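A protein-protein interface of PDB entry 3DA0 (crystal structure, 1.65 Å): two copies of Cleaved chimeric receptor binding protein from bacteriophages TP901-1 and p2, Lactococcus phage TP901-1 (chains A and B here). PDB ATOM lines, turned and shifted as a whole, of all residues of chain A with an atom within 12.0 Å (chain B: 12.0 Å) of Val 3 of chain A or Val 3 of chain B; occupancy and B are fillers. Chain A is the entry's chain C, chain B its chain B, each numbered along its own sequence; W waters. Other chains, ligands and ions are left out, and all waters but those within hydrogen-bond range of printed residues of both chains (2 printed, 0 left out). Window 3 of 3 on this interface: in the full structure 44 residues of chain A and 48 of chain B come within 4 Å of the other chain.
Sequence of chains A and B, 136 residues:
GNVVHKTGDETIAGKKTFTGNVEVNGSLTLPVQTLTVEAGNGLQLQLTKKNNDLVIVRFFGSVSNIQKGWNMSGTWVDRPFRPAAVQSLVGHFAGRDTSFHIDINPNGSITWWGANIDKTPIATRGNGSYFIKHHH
The backbone carbonyl oxygen (O) of Val 3 of chain B sits close to a ring nitrogen (ND1) of His 5 of chain B (3.2 Å).
The side-chain carboxylate (OE2) of Glu 10 of chain B sits at hydrogen-bond distance from a ring nitrogen (ND1) of His 5 of chain B, 2.7 Å away.
NZ of Lys 16 of chain B sits close to O of Ala 13 of chain B (3.4 Å).
The backbone carbonyl oxygen (O) of Val 3 of chain A lies within hydrogen-bond range of a ring nitrogen (ND1) of His 5 of chain A, at 3.0 Å.
A ring nitrogen (ND1) of His 5 of chain A sits at hydrogen-bond distance from the side-chain carboxylate (OE2) of Glu 10 of chain A (2.8 Å).
O of Ala 13 of chain A lies close to NZ of Lys 16 of chain A.
Lys 6 of chain A touches Asn 2 of chain B, but with the chains exchanged Asn 2 of chain A does not touch Lys 6 of chain B (9.3 Å).
Thr 7 of chain A touches Lys 16 of chain B, but with the chains exchanged Lys 16 of chain A does not touch Thr 7 of chain B (11.7 Å).
Gly 8 of chain A touches Ala 13 of chain B, but with the chains exchanged Ala 13 of chain A does not touch Gly 8 of chain B (17.6 Å).
Gly 8 of chain A touches Gly 14 of chain B, but with the chains exchanged Gly 14 of chain A does not touch Gly 8 of chain B (17.4 Å).
The backbone NH of Lys 6 of chain A sits at hydrogen-bond distance from the backbone carbonyl oxygen of Asn 2 of chain B (3.0 Å).
The side-chain amide oxygen of Asn 2 of chain B sits close to the side-chain hydroxyl of Thr 7 of chain A (3.3 Å).
The backbone carbonyl oxygen (O) of Val 4 of chain A sits at hydrogen-bond distance from the backbone NH (N) of Val 4 of chain B (2.9 Å).
OE2 of Glu 10 of chain B lies within salt-bridge range of NZ of Lys 6 of chain A, at 3.4 Å.
O of Lys 6 of chain A lies within hydrogen-bond range of N of Ala 13 of chain B (2.8 Å).
The side-chain carboxylate (OD1) of Asp 9 of chain A is in hydrogen-bond range of the backbone NH (N) of Lys 15 of chain B (2.9 Å).
O of Lys 15 of chain B lies within hydrogen-bond range of N of Glu 10 of chain A (2.8 Å).
O of His 5 of chain A sits at hydrogen-bond distance from NZ of Lys 16 of chain B, at 2.8 Å.
The side-chain amino group (NZ) of Lys 16 of chain B is in hydrogen-bond range of the backbone carbonyl oxygen (O) of Thr 7 of chain A (3.1 Å).
The side-chain amino group (NZ) of Lys 16 of chain B sits at hydrogen-bond distance from the backbone carbonyl oxygen (O) of Gly 8 of chain A (2.7 Å).
The side-chain carboxylate (OE1) of Glu 10 of chain A lies within salt-bridge range of the side-chain amino group (NZ) of Lys 16 of chain B, 2.6 Å away.
The backbone NH of Thr 17 of chain B sits at hydrogen-bond distance from the backbone carbonyl oxygen of Glu 10 of chain A (2.8 Å).
N of Ile 12 of chain A is in hydrogen-bond range of O of Thr 17 of chain B, 2.6 Å away.
No residue of chain B comes within 4 Å of Gly 1 of chain A.
No residue of chain B comes within 4 Å of Asn 2 of chain A.
Val 3 of chain A touches just one residue of chain B: Val 3.
Val 4 of chain A touches just these residues of chain B: Val 3 (3.5 Å) and Val 4 (2.9 Å).
His 5 of chain A touches just these residues of chain B: Asn 2, Val 4, Ile 12 and Lys 16.
Lys 6 of chain A touches just these residues of chain B: Asn 2 (3.0 Å), Val 3 (3.6 Å), Glu 10 (3.1 Å), Thr 11 (3.5 Å), Ile 12 (3.8 Å) and Ala 13 (2.8 Å).
Printed residues of chain B within 4 Å of Asp 9 of chain A: Gly 14 (3.8 Å) and Lys 15 (2.9 Å).
Ala 13 of chain A touches none of the printed residues of chain B.
Val 3 of chain B touches three residues of chain A.
Val 4 of chain B touches just these residues of chain A: Val 4 (2.9 Å) and His 5 (3.9 Å).
No residue of chain A comes within 4 Å of His 5 of chain B.
Of the printed residues of chain A, Glu 10 of chain B touches Lys 6 (3.1 Å).
Printed residues of chain A within 4 Å of Ile 12 of chain B: His 5 (3.9 Å) and Lys 6 (3.8 Å).
Printed residues of chain A within 4 Å of Phe 18 of chain B: Ile 12 (3.3 Å) and Lys 16 (3.8 Å).
The nearest residue of chain B that does not touch Val 3 of chain A is Val 4 of chain B (6.0 Å).
The nearest residue of chain A that does not touch Val 3 of chain B is His 5 of chain A (4.2 Å).
Water W1 lies within hydrogen-bond range of O of Lys 15 of chain B (2.8 Å), OG1 of Thr 17 of chain B (2.8 Å) and O of Glu 10 of chain A (3.3 Å).
Water W2 lies within hydrogen-bond range of N of Thr 11 of chain B (2.9 Å) and NZ of Lys 6 of chain A (2.9 Å).
Val 3 of chain B touches Val 3 of chain A (CG2 to CG2, 3.8 Å).
CA of Val 3 of chain B touches O of Val 4 of chain A, at 3.5 Å.
CG2 of Val 4 of chain B touches O of His 5 of chain A (3.9 Å).
Ile 12 of chain B touches His 5 of chain A (CG2 to O, 3.9 Å).
Val 3 of chain B touches Lys 6 of chain A (O to CE, 3.6 Å).
CB of Lys 6 of chain A touches O of Thr 11 of chain B, at 3.5 Å.
C of Ile 12 of chain B touches O of Lys 6 of chain A, 3.8 Å away.
Gly 8 of chain A touches Ala 13 of chain B (O to O, 3.7 Å).
Thr 11 of chain A touches Thr 17 of chain B.
Phe 18 of chain B touches Ile 12 of chain A.
Of the 17 printed residues of chain B, 12 touch a printed residue of chain A.
Hydrophobic or aromatic side chains of chain B that line the printed part of chain A: Val 3, Val 4, Ile 12, Ala 13 and Phe 18.
Among the printed residues, Asp or Glu carboxylates within 4 Å of a Lys or Arg side-chain nitrogen of the other chain: Lys 6 of chain A with Glu 10 of chain B and Glu 10 of chain A with Lys 16 of chain B.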
ATOM      1  N   GLY A   1       3.012  34.706  -3.045  1.00  0.00           N
ATOM      2  CA  GLY A   1       3.938  34.453  -1.927  1.00  0.00           C
ATOM      3  C   GLY A   1       5.345  34.694  -2.456  1.00  0.00           C
ATOM      4  O   GLY A   1       5.713  34.137  -3.500  1.00  0.00           O
ATOM      5  N   ASN A   2       6.123  35.487  -1.724  1.00  0.00           N
ATOM      6  CA  ASN A   2       7.452  35.867  -2.138  1.00  0.00           C
ATOM      7  C   ASN A   2       8.574  35.257  -1.284  1.00  0.00           C
ATOM      8  O   ASN A   2       9.567  35.908  -1.032  1.00  0.00           O
ATOM      9  CB  ASN A   2       7.559  37.374  -2.065  1.00  0.00           C
ATOM     10  CG  ASN A   2       8.772  37.882  -2.767  1.00  0.00           C
ATOM     11  OD1 ASN A   2       9.174  37.299  -3.748  1.00  0.00           O
ATOM     12  ND2 ASN A   2       9.365  38.966  -2.276  1.00  0.00           N
ATOM     13  N   VAL A   3       8.383  34.032  -0.812  1.00  0.00           N
ATOM     14  CA  VAL A   3       9.359  33.377   0.063  1.00  0.00           C
ATOM     15  C   VAL A   3       9.966  32.154  -0.633  1.00  0.00           C
ATOM     16  O   VAL A   3       9.291  31.501  -1.421  1.00  0.00           O
ATOM     17  CB  VAL A   3       8.732  32.945   1.375  1.00  0.00           C
ATOM     18  CG1 VAL A   3       8.111  34.133   2.059  1.00  0.00           C
ATOM     19  CG2 VAL A   3       7.683  31.849   1.148  1.00  0.00           C
ATOM     20  N   VAL A   4      11.226  31.862  -0.338  1.00  0.00           N
ATOM     21  CA  VAL A   4      11.858  30.623  -0.772  1.00  0.00           C
ATOM     22  C   VAL A   4      11.388  29.442   0.068  1.00  0.00           C
ATOM     23  O   VAL A   4      11.384  29.483   1.293  1.00  0.00           O
ATOM     24  CB  VAL A   4      13.400  30.716  -0.677  1.00  0.00           C
ATOM     25  CG1 VAL A   4      14.049  29.409  -1.146  1.00  0.00           C
ATOM     26  CG2 VAL A   4      13.927  31.880  -1.525  1.00  0.00           C
ATOM     27  N   HIS A   5      11.036  28.367  -0.617  1.00  0.00           N
ATOM     28  CA  HIS A   5      10.566  27.141   0.008  1.00  0.00           C
ATOM     29  C   HIS A   5      11.607  26.042   0.035  1.00  0.00           C
ATOM     30  O   HIS A   5      12.531  26.054  -0.765  1.00  0.00           O
ATOM     31  CB  HIS A   5       9.347  26.646  -0.740  1.00  0.00           C
ATOM     32  CG  HIS A   5       8.189  27.576  -0.626  1.00  0.00           C
ATOM     33  ND1 HIS A   5       8.088  28.726  -1.379  1.00  0.00           N
ATOM     34  CD2 HIS A   5       7.123  27.568   0.203  1.00  0.00           C
ATOM     35  CE1 HIS A   5       6.983  29.368  -1.044  1.00  0.00           C
ATOM     36  NE2 HIS A   5       6.382  28.684  -0.087  1.00  0.00           N
ATOM     37  N   LYS A   6      11.443  25.083   0.954  1.00  0.00           N
ATOM     38  CA  LYS A   6      12.417  23.991   1.095  1.00  0.00           C
ATOM     39  C   LYS A   6      12.092  22.884   0.119  1.00  0.00           C
ATOM     40  O   LYS A   6      12.705  21.805   0.141  1.00  0.00           O
ATOM     41  CB  LYS A   6      12.442  23.420   2.496  1.00  0.00           C
ATOM     42  CG  LYS A   6      12.846  24.383   3.528  1.00  0.00           C
ATOM     43  CD  LYS A   6      12.683  23.714   4.866  1.00  0.00           C
ATOM     44  CE  LYS A   6      13.480  24.373   5.886  1.00  0.00           C
ATOM     45  NZ  LYS A   6      13.159  23.704   7.174  1.00  0.00           N
ATOM     46  N   THR A   7      11.132  23.146  -0.748  1.00  0.00           N
ATOM     47  CA  THR A   7      10.842  22.242  -1.845  1.00  0.00           C
ATOM     48  C   THR A   7      10.523  23.087  -3.062  1.00  0.00           C
ATOM     49  O   THR A   7      10.288  24.277  -2.953  1.00  0.00           O
ATOM     50  CB  THR A   7       9.630  21.354  -1.511  1.00  0.00           C
ATOM     51  OG1 THR A   7       8.478  22.182  -1.514  1.00  0.00           O
ATOM     52  CG2 THR A   7       9.782  20.715  -0.126  1.00  0.00           C
ATOM     53  N   GLY A   8      10.525  22.460  -4.228  1.00  0.00           N
ATOM     54  CA  GLY A   8      10.040  23.106  -5.449  1.00  0.00           C
ATOM     55  C   GLY A   8      11.124  23.837  -6.197  1.00  0.00           C
ATOM     56  O   GLY A   8      12.102  24.288  -5.611  1.00  0.00           O
ATOM     57  N   ASP A   9      10.937  23.938  -7.511  1.00  0.00           N
ATOM     58  CA  ASP A   9      11.825  24.668  -8.364  1.00  0.00           C
ATOM     59  C   ASP A   9      11.406  26.118  -8.249  1.00  0.00           C
ATOM     60  O   ASP A   9      10.230  26.458  -8.389  1.00  0.00           O
ATOM     61  CB  ASP A   9      11.688  24.211  -9.809  1.00  0.00           C
ATOM     62  CG  ASP A   9      12.206  22.789 -10.031  1.00  0.00           C
ATOM     63  OD1 ASP A   9      12.685  22.118  -9.083  1.00  0.00           O
ATOM     64  OD2 ASP A   9      12.141  22.340 -11.192  1.00  0.00           O
ATOM     65  N   GLU A  10      12.370  26.985  -8.023  1.00  0.00           N
ATOM     66  CA  GLU A  10      12.111  28.386  -7.741  1.00  0.00           C
ATOM     67  C   GLU A  10      13.221  29.264  -8.290  1.00  0.00           C
ATOM     68  O   GLU A  10      14.382  28.904  -8.304  1.00  0.00           O
ATOM     69  CB  GLU A  10      12.020  28.580  -6.237  1.00  0.00           C
ATOM     70  CG  GLU A  10      10.735  28.059  -5.654  1.00  0.00           C
ATOM     71  CD  GLU A  10      10.629  28.299  -4.154  1.00  0.00           C
ATOM     72  OE1 GLU A  10      11.594  27.968  -3.429  1.00  0.00           O
ATOM     73  OE2 GLU A  10       9.563  28.802  -3.704  1.00  0.00           O
ATOM     74  N   THR A  11      12.830  30.428  -8.753  1.00  0.00           N
ATOM     75  CA  THR A  11      13.737  31.416  -9.222  1.00  0.00           C
ATOM     76  C   THR A  11      13.753  32.536  -8.167  1.00  0.00           C
ATOM     77  O   THR A  11      12.718  32.948  -7.649  1.00  0.00           O
ATOM     78  CB  THR A  11      13.287  31.869 -10.626  1.00  0.00           C
ATOM     79  OG1 THR A  11      13.336  30.739 -11.521  1.00  0.00           O
ATOM     80  CG2 THR A  11      14.126  32.894 -11.172  1.00  0.00           C
ATOM     81  N   ILE A  12      14.948  33.015  -7.866  1.00  0.00           N
ATOM     82  CA  ILE A  12      15.210  33.841  -6.678  1.00  0.00           C
ATOM     83  C   ILE A  12      16.066  35.039  -7.082  1.00  0.00           C
ATOM     84  O   ILE A  12      17.202  34.866  -7.510  1.00  0.00           O
ATOM     85  CB  ILE A  12      15.988  33.043  -5.592  1.00  0.00           C
ATOM     86  CG1 ILE A  12      15.205  31.799  -5.196  1.00  0.00           C
ATOM     87  CG2 ILE A  12      16.299  33.922  -4.388  1.00  0.00           C
ATOM     88  CD1 ILE A  12      16.034  30.792  -4.446  1.00  0.00           C
ATOM     89  N   ALA A  13      15.506  36.242  -6.972  1.00  0.00           N
ATOM     90  CA  ALA A  13      16.243  37.475  -7.237  1.00  0.00           C
ATOM     91  C   ALA A  13      16.759  38.064  -5.926  1.00  0.00           C
ATOM     92  O   ALA A  13      16.319  37.656  -4.868  1.00  0.00           O
ATOM     93  CB  ALA A  13      15.353  38.488  -7.935  1.00  0.00           C
ATOM     94  N   GLY A  14      17.697  38.998  -6.054  1.00  0.00           N
ATOM     95  CA  GLY A  14      18.341  39.663  -4.932  1.00  0.00           C
ATOM     96  C   GLY A  14      19.723  39.072  -4.704  1.00  0.00           C
ATOM     97  O   GLY A  14      19.992  37.888  -5.005  1.00  0.00           O
ATOM     98  N   LYS A  16      21.968  37.321  -2.511  1.00  0.00           N
ATOM     99  CA  LYS A  16      21.834  36.512  -1.336  1.00  0.00           C
ATOM    100  C   LYS A  16      23.239  36.230  -0.819  1.00  0.00           C
ATOM    101  O   LYS A  16      24.045  35.584  -1.458  1.00  0.00           O
ATOM    102  CB  LYS A  16      21.061  35.227  -1.656  1.00  0.00           C
ATOM    103  CG  LYS A  16      19.699  35.426  -2.257  1.00  0.00           C
ATOM    104  CD  LYS A  16      18.765  36.384  -1.471  1.00  0.00           C
ATOM    105  CE  LYS A  16      17.404  36.410  -2.148  1.00  0.00           C
ATOM    106  NZ  LYS A  16      16.431  37.443  -1.627  1.00  0.00           N
ATOM    107  N   PHE A  18      25.191  34.316   1.929  1.00  0.00           N
ATOM    108  CA  PHE A  18      25.131  33.233   2.884  1.00  0.00           C
ATOM    109  C   PHE A  18      26.347  33.411   3.772  1.00  0.00           C
ATOM    110  O   PHE A  18      27.478  33.210   3.348  1.00  0.00           O
ATOM    111  CB  PHE A  18      25.164  31.889   2.170  1.00  0.00           C
ATOM    112  CG  PHE A  18      23.937  31.622   1.387  1.00  0.00           C
ATOM    113  CD1 PHE A  18      23.847  32.064   0.065  1.00  0.00           C
ATOM    114  CD2 PHE A  18      22.868  30.958   1.956  1.00  0.00           C
ATOM    115  CE1 PHE A  18      22.716  31.829  -0.642  1.00  0.00           C
ATOM    116  CE2 PHE A  18      21.711  30.715   1.243  1.00  0.00           C
ATOM    117  CZ  PHE A  18      21.607  31.170  -0.021  1.00  0.00           C
ATOM    118  N   ASN B   2       7.928  24.804   5.627  1.00  0.00           N
ATOM    119  CA  ASN B   2       8.411  24.582   4.237  1.00  0.00           C
ATOM    120  C   ASN B   2       9.075  25.849   3.693  1.00  0.00           C
ATOM    121  O   ASN B   2       9.061  26.088   2.499  1.00  0.00           O
ATOM    122  CB  ASN B   2       7.249  24.145   3.336  1.00  0.00           C
ATOM    123  CG  ASN B   2       7.701  23.807   1.889  1.00  0.00           C
ATOM    124  OD1 ASN B   2       8.634  23.023   1.672  1.00  0.00           O
ATOM    125  ND2 ASN B   2       7.020  24.396   0.908  1.00  0.00           N
ATOM    126  N   VAL B   3       9.609  26.673   4.583  1.00  0.00           N
ATOM    127  CA  VAL B   3      10.116  27.988   4.212  1.00  0.00           C
ATOM    128  C   VAL B   3      11.577  28.095   4.659  1.00  0.00           C
ATOM    129  O   VAL B   3      11.943  27.570   5.691  1.00  0.00           O
ATOM    130  CB  VAL B   3       9.243  29.091   4.829  1.00  0.00           C
ATOM    131  CG1 VAL B   3       9.990  30.389   4.938  1.00  0.00           C
ATOM    132  CG2 VAL B   3       7.984  29.278   3.996  1.00  0.00           C
ATOM    133  N   VAL B   4      12.427  28.710   3.837  1.00  0.00           N
ATOM    134  CA  VAL B   4      13.832  28.908   4.196  1.00  0.00           C
ATOM    135  C   VAL B   4      13.983  30.155   5.037  1.00  0.00           C
ATOM    136  O   VAL B   4      13.494  31.210   4.670  1.00  0.00           O
ATOM    137  CB  VAL B   4      14.696  29.049   2.951  1.00  0.00           C
ATOM    138  CG1 VAL B   4      16.179  29.156   3.328  1.00  0.00           C
ATOM    139  CG2 VAL B   4      14.451  27.847   2.053  1.00  0.00           C
ATOM    140  N   HIS B   5      14.680  30.031   6.164  1.00  0.00           N
ATOM    141  CA  HIS B   5      14.866  31.153   7.068  1.00  0.00           C
ATOM    142  C   HIS B   5      16.266  31.727   7.020  1.00  0.00           C
ATOM    143  O   HIS B   5      17.205  31.084   6.560  1.00  0.00           O
ATOM    144  CB  HIS B   5      14.582  30.723   8.507  1.00  0.00           C
ATOM    145  CG  HIS B   5      13.233  30.086   8.694  1.00  0.00           C
ATOM    146  ND1 HIS B   5      13.007  28.740   8.491  1.00  0.00           N
ATOM    147  CD2 HIS B   5      12.043  30.616   9.060  1.00  0.00           C
ATOM    148  CE1 HIS B   5      11.736  28.468   8.738  1.00  0.00           C
ATOM    149  NE2 HIS B   5      11.127  29.591   9.072  1.00  0.00           N
ATOM    150  N   LYS B   6      16.393  32.937   7.547  1.00  0.00           N
ATOM    151  CA  LYS B   6      17.667  33.649   7.578  1.00  0.00           C
ATOM    152  C   LYS B   6      18.579  33.187   8.729  1.00  0.00           C
ATOM    153  O   LYS B   6      19.654  33.718   8.927  1.00  0.00           O
ATOM    154  CB  LYS B   6      17.434  35.160   7.646  1.00  0.00           C
ATOM    155  CG  LYS B   6      17.003  35.821   6.336  1.00  0.00           C
ATOM    156  CD  LYS B   6      16.591  37.292   6.573  1.00  0.00           C
ATOM    157  CE  LYS B   6      16.151  37.950   5.263  1.00  0.00           C
ATOM    158  NZ  LYS B   6      15.461  39.287   5.376  1.00  0.00           N
ATOM    159  N   THR B   7      18.157  32.152   9.423  1.00  0.00           N
ATOM    160  CA  THR B   7      18.969  31.521  10.433  1.00  0.00           C
ATOM    161  C   THR B   7      18.703  30.052  10.366  1.00  0.00           C
ATOM    162  O   THR B   7      17.706  29.635   9.768  1.00  0.00           O
ATOM    163  CB  THR B   7      18.632  32.016  11.863  1.00  0.00           C
ATOM    164  OG1 THR B   7      17.260  31.739  12.162  1.00  0.00           O
ATOM    165  CG2 THR B   7      18.877  33.543  11.996  1.00  0.00           C
ATOM    166  N   GLY B   8      19.578  29.283  11.007  1.00  0.00           N
ATOM    167  CA  GLY B   8      19.383  27.857  11.196  1.00  0.00           C
ATOM    168  C   GLY B   8      19.847  26.962  10.074  1.00  0.00           C
ATOM    169  O   GLY B   8      19.890  27.389   8.918  1.00  0.00           O
ATOM    170  N   ASP B   9      20.193  25.727  10.434  1.00  0.00           N
ATOM    171  CA  ASP B   9      20.565  24.679   9.482  1.00  0.00           C
ATOM    172  C   ASP B   9      19.333  24.079   8.838  1.00  0.00           C
ATOM    173  O   ASP B   9      18.442  23.601   9.512  1.00  0.00           O
ATOM    174  CB  ASP B   9      21.343  23.577  10.208  1.00  0.00           C
ATOM    175  CG  ASP B   9      22.689  24.071  10.761  1.00  0.00           C
ATOM    176  OD1 ASP B   9      23.014  25.279  10.603  1.00  0.00           O
ATOM    177  OD2 ASP B   9      23.407  23.243  11.397  1.00  0.00           O
ATOM    178  N   GLU B  10      19.283  24.100   7.524  1.00  0.00           N
ATOM    179  CA  GLU B  10      18.110  23.700   6.823  1.00  0.00           C
ATOM    180  C   GLU B  10      18.502  22.975   5.564  1.00  0.00           C
ATOM    181  O   GLU B  10      19.556  23.255   4.977  1.00  0.00           O
ATOM    182  CB  GLU B  10      17.277  24.937   6.467  1.00  0.00           C
ATOM    183  CG  GLU B  10      16.693  25.700   7.676  1.00  0.00           C
ATOM    184  CD  GLU B  10      15.767  26.815   7.277  1.00  0.00           C
ATOM    185  OE1 GLU B  10      16.221  27.733   6.569  1.00  0.00           O
ATOM    186  OE2 GLU B  10      14.551  26.755   7.624  1.00  0.00           O
ATOM    187  N   THR B  11      17.618  22.092   5.131  1.00  0.00           N
ATOM    188  CA  THR B  11      17.760  21.364   3.875  1.00  0.00           C
ATOM    189  C   THR B  11      16.738  21.910   2.924  1.00  0.00           C
ATOM    190  O   THR B  11      15.554  22.071   3.276  1.00  0.00           O
ATOM    191  CB  THR B  11      17.470  19.878   4.067  1.00  0.00           C
ATOM    192  OG1 THR B  11      18.417  19.334   4.994  1.00  0.00           O
ATOM    193  CG2 THR B  11      17.529  19.136   2.728  1.00  0.00           C
ATOM    194  N   ILE B  12      17.186  22.110   1.699  1.00  0.00           N
ATOM    195  CA  ILE B  12      16.437  22.823   0.694  1.00  0.00           C
ATOM    196  C   ILE B  12      16.430  21.981  -0.572  1.00  0.00           C
ATOM    197  O   ILE B  12      17.451  21.848  -1.233  1.00  0.00           O
ATOM    198  CB  ILE B  12      17.078  24.212   0.421  1.00  0.00           C
ATOM    199  CG1 ILE B  12      17.152  25.050   1.693  1.00  0.00           C
ATOM    200  CG2 ILE B  12      16.336  25.018  -0.674  1.00  0.00           C
ATOM    201  CD1 ILE B  12      17.900  26.355   1.446  1.00  0.00           C
ATOM    202  N   ALA B  13      15.261  21.462  -0.917  1.00  0.00           N
ATOM    203  CA  ALA B  13      15.084  20.624  -2.090  1.00  0.00           C
ATOM    204  C   ALA B  13      14.567  21.503  -3.204  1.00  0.00           C
ATOM    205  O   ALA B  13      14.102  22.601  -2.949  1.00  0.00           O
ATOM    206  CB  ALA B  13      14.081  19.521  -1.771  1.00  0.00           C
ATOM    207  N   GLY B  14      14.679  21.030  -4.446  1.00  0.00           N
ATOM    208  CA  GLY B  14      14.177  21.775  -5.600  1.00  0.00           C
ATOM    209  C   GLY B  14      15.293  22.474  -6.344  1.00  0.00           C
ATOM    210  O   GLY B  14      16.321  22.799  -5.771  1.00  0.00           O
ATOM    211  N   LYS B  15      15.070  22.723  -7.632  1.00  0.00           N
ATOM    212  CA  LYS B  15      16.016  23.477  -8.421  1.00  0.00           C
ATOM    213  C   LYS B  15      15.845  24.954  -8.042  1.00  0.00           C
ATOM    214  O   LYS B  15      14.816  25.545  -8.258  1.00  0.00           O
ATOM    215  CB  LYS B  15      15.724  23.265  -9.915  1.00  0.00           C
ATOM    216  CG  LYS B  15      16.623  24.034 -10.902  1.00  0.00           C
ATOM    217  CD  LYS B  15      15.926  24.040 -12.305  1.00  0.00           C
ATOM    218  CE  LYS B  15      16.709  24.873 -13.323  1.00  0.00           C
ATOM    219  NZ  LYS B  15      15.885  25.257 -14.529  1.00  0.00           N
ATOM    220  N   LYS B  16      16.882  25.536  -7.461  1.00  0.00           N
ATOM    221  CA  LYS B  16      16.839  26.910  -7.046  1.00  0.00           C
ATOM    222  C   LYS B  16      17.733  27.693  -7.982  1.00  0.00           C
ATOM    223  O   LYS B  16      18.914  27.447  -8.072  1.00  0.00           O
ATOM    224  CB  LYS B  16      17.295  27.077  -5.601  1.00  0.00           C
ATOM    225  CG  LYS B  16      16.491  26.240  -4.627  1.00  0.00           C
ATOM    226  CD  LYS B  16      15.020  26.465  -4.613  1.00  0.00           C
ATOM    227  CE  LYS B  16      14.421  25.818  -3.363  1.00  0.00           C
ATOM    228  NZ  LYS B  16      12.934  25.762  -3.517  1.00  0.00           N
ATOM    229  N   THR B  17      17.155  28.677  -8.638  1.00  0.00           N
ATOM    230  CA  THR B  17      17.900  29.519  -9.573  1.00  0.00           C
ATOM    231  C   THR B  17      18.003  30.933  -8.994  1.00  0.00           C
ATOM    232  O   THR B  17      16.979  31.627  -8.794  1.00  0.00           O
ATOM    233  CB  THR B  17      17.185  29.591 -10.943  1.00  0.00           C
ATOM    234  OG1 THR B  17      17.096  28.264 -11.503  1.00  0.00           O
ATOM    235  CG2 THR B  17      17.950  30.460 -11.902  1.00  0.00           C
ATOM    236  N   PHE B  18      19.236  31.344  -8.703  1.00  0.00           N
ATOM    237  CA  PHE B  18      19.516  32.690  -8.206  1.00  0.00           C
ATOM    238  C   PHE B  18      19.852  33.521  -9.423  1.00  0.00           C
ATOM    239  O   PHE B  18      20.848  33.294 -10.065  1.00  0.00           O
ATOM    240  CB  PHE B  18      20.657  32.683  -7.207  1.00  0.00           C
ATOM    241  CG  PHE B  18      20.327  31.928  -5.958  1.00  0.00           C
ATOM    242  CD1 PHE B  18      20.520  30.571  -5.918  1.00  0.00           C
ATOM    243  CD2 PHE B  18      19.882  32.585  -4.819  1.00  0.00           C
ATOM    244  CE1 PHE B  18      20.239  29.839  -4.756  1.00  0.00           C
ATOM    245  CE2 PHE B  18      19.566  31.871  -3.644  1.00  0.00           C
ATOM    246  CZ  PHE B  18      19.767  30.496  -3.621  1.00  0.00           C
HETATM  247  O   HOH W   1      14.813  26.741 -10.759  1.00  0.00           O
HETATM  248  O   HOH W   2      15.344  21.823   6.872  1.00  0.00           O
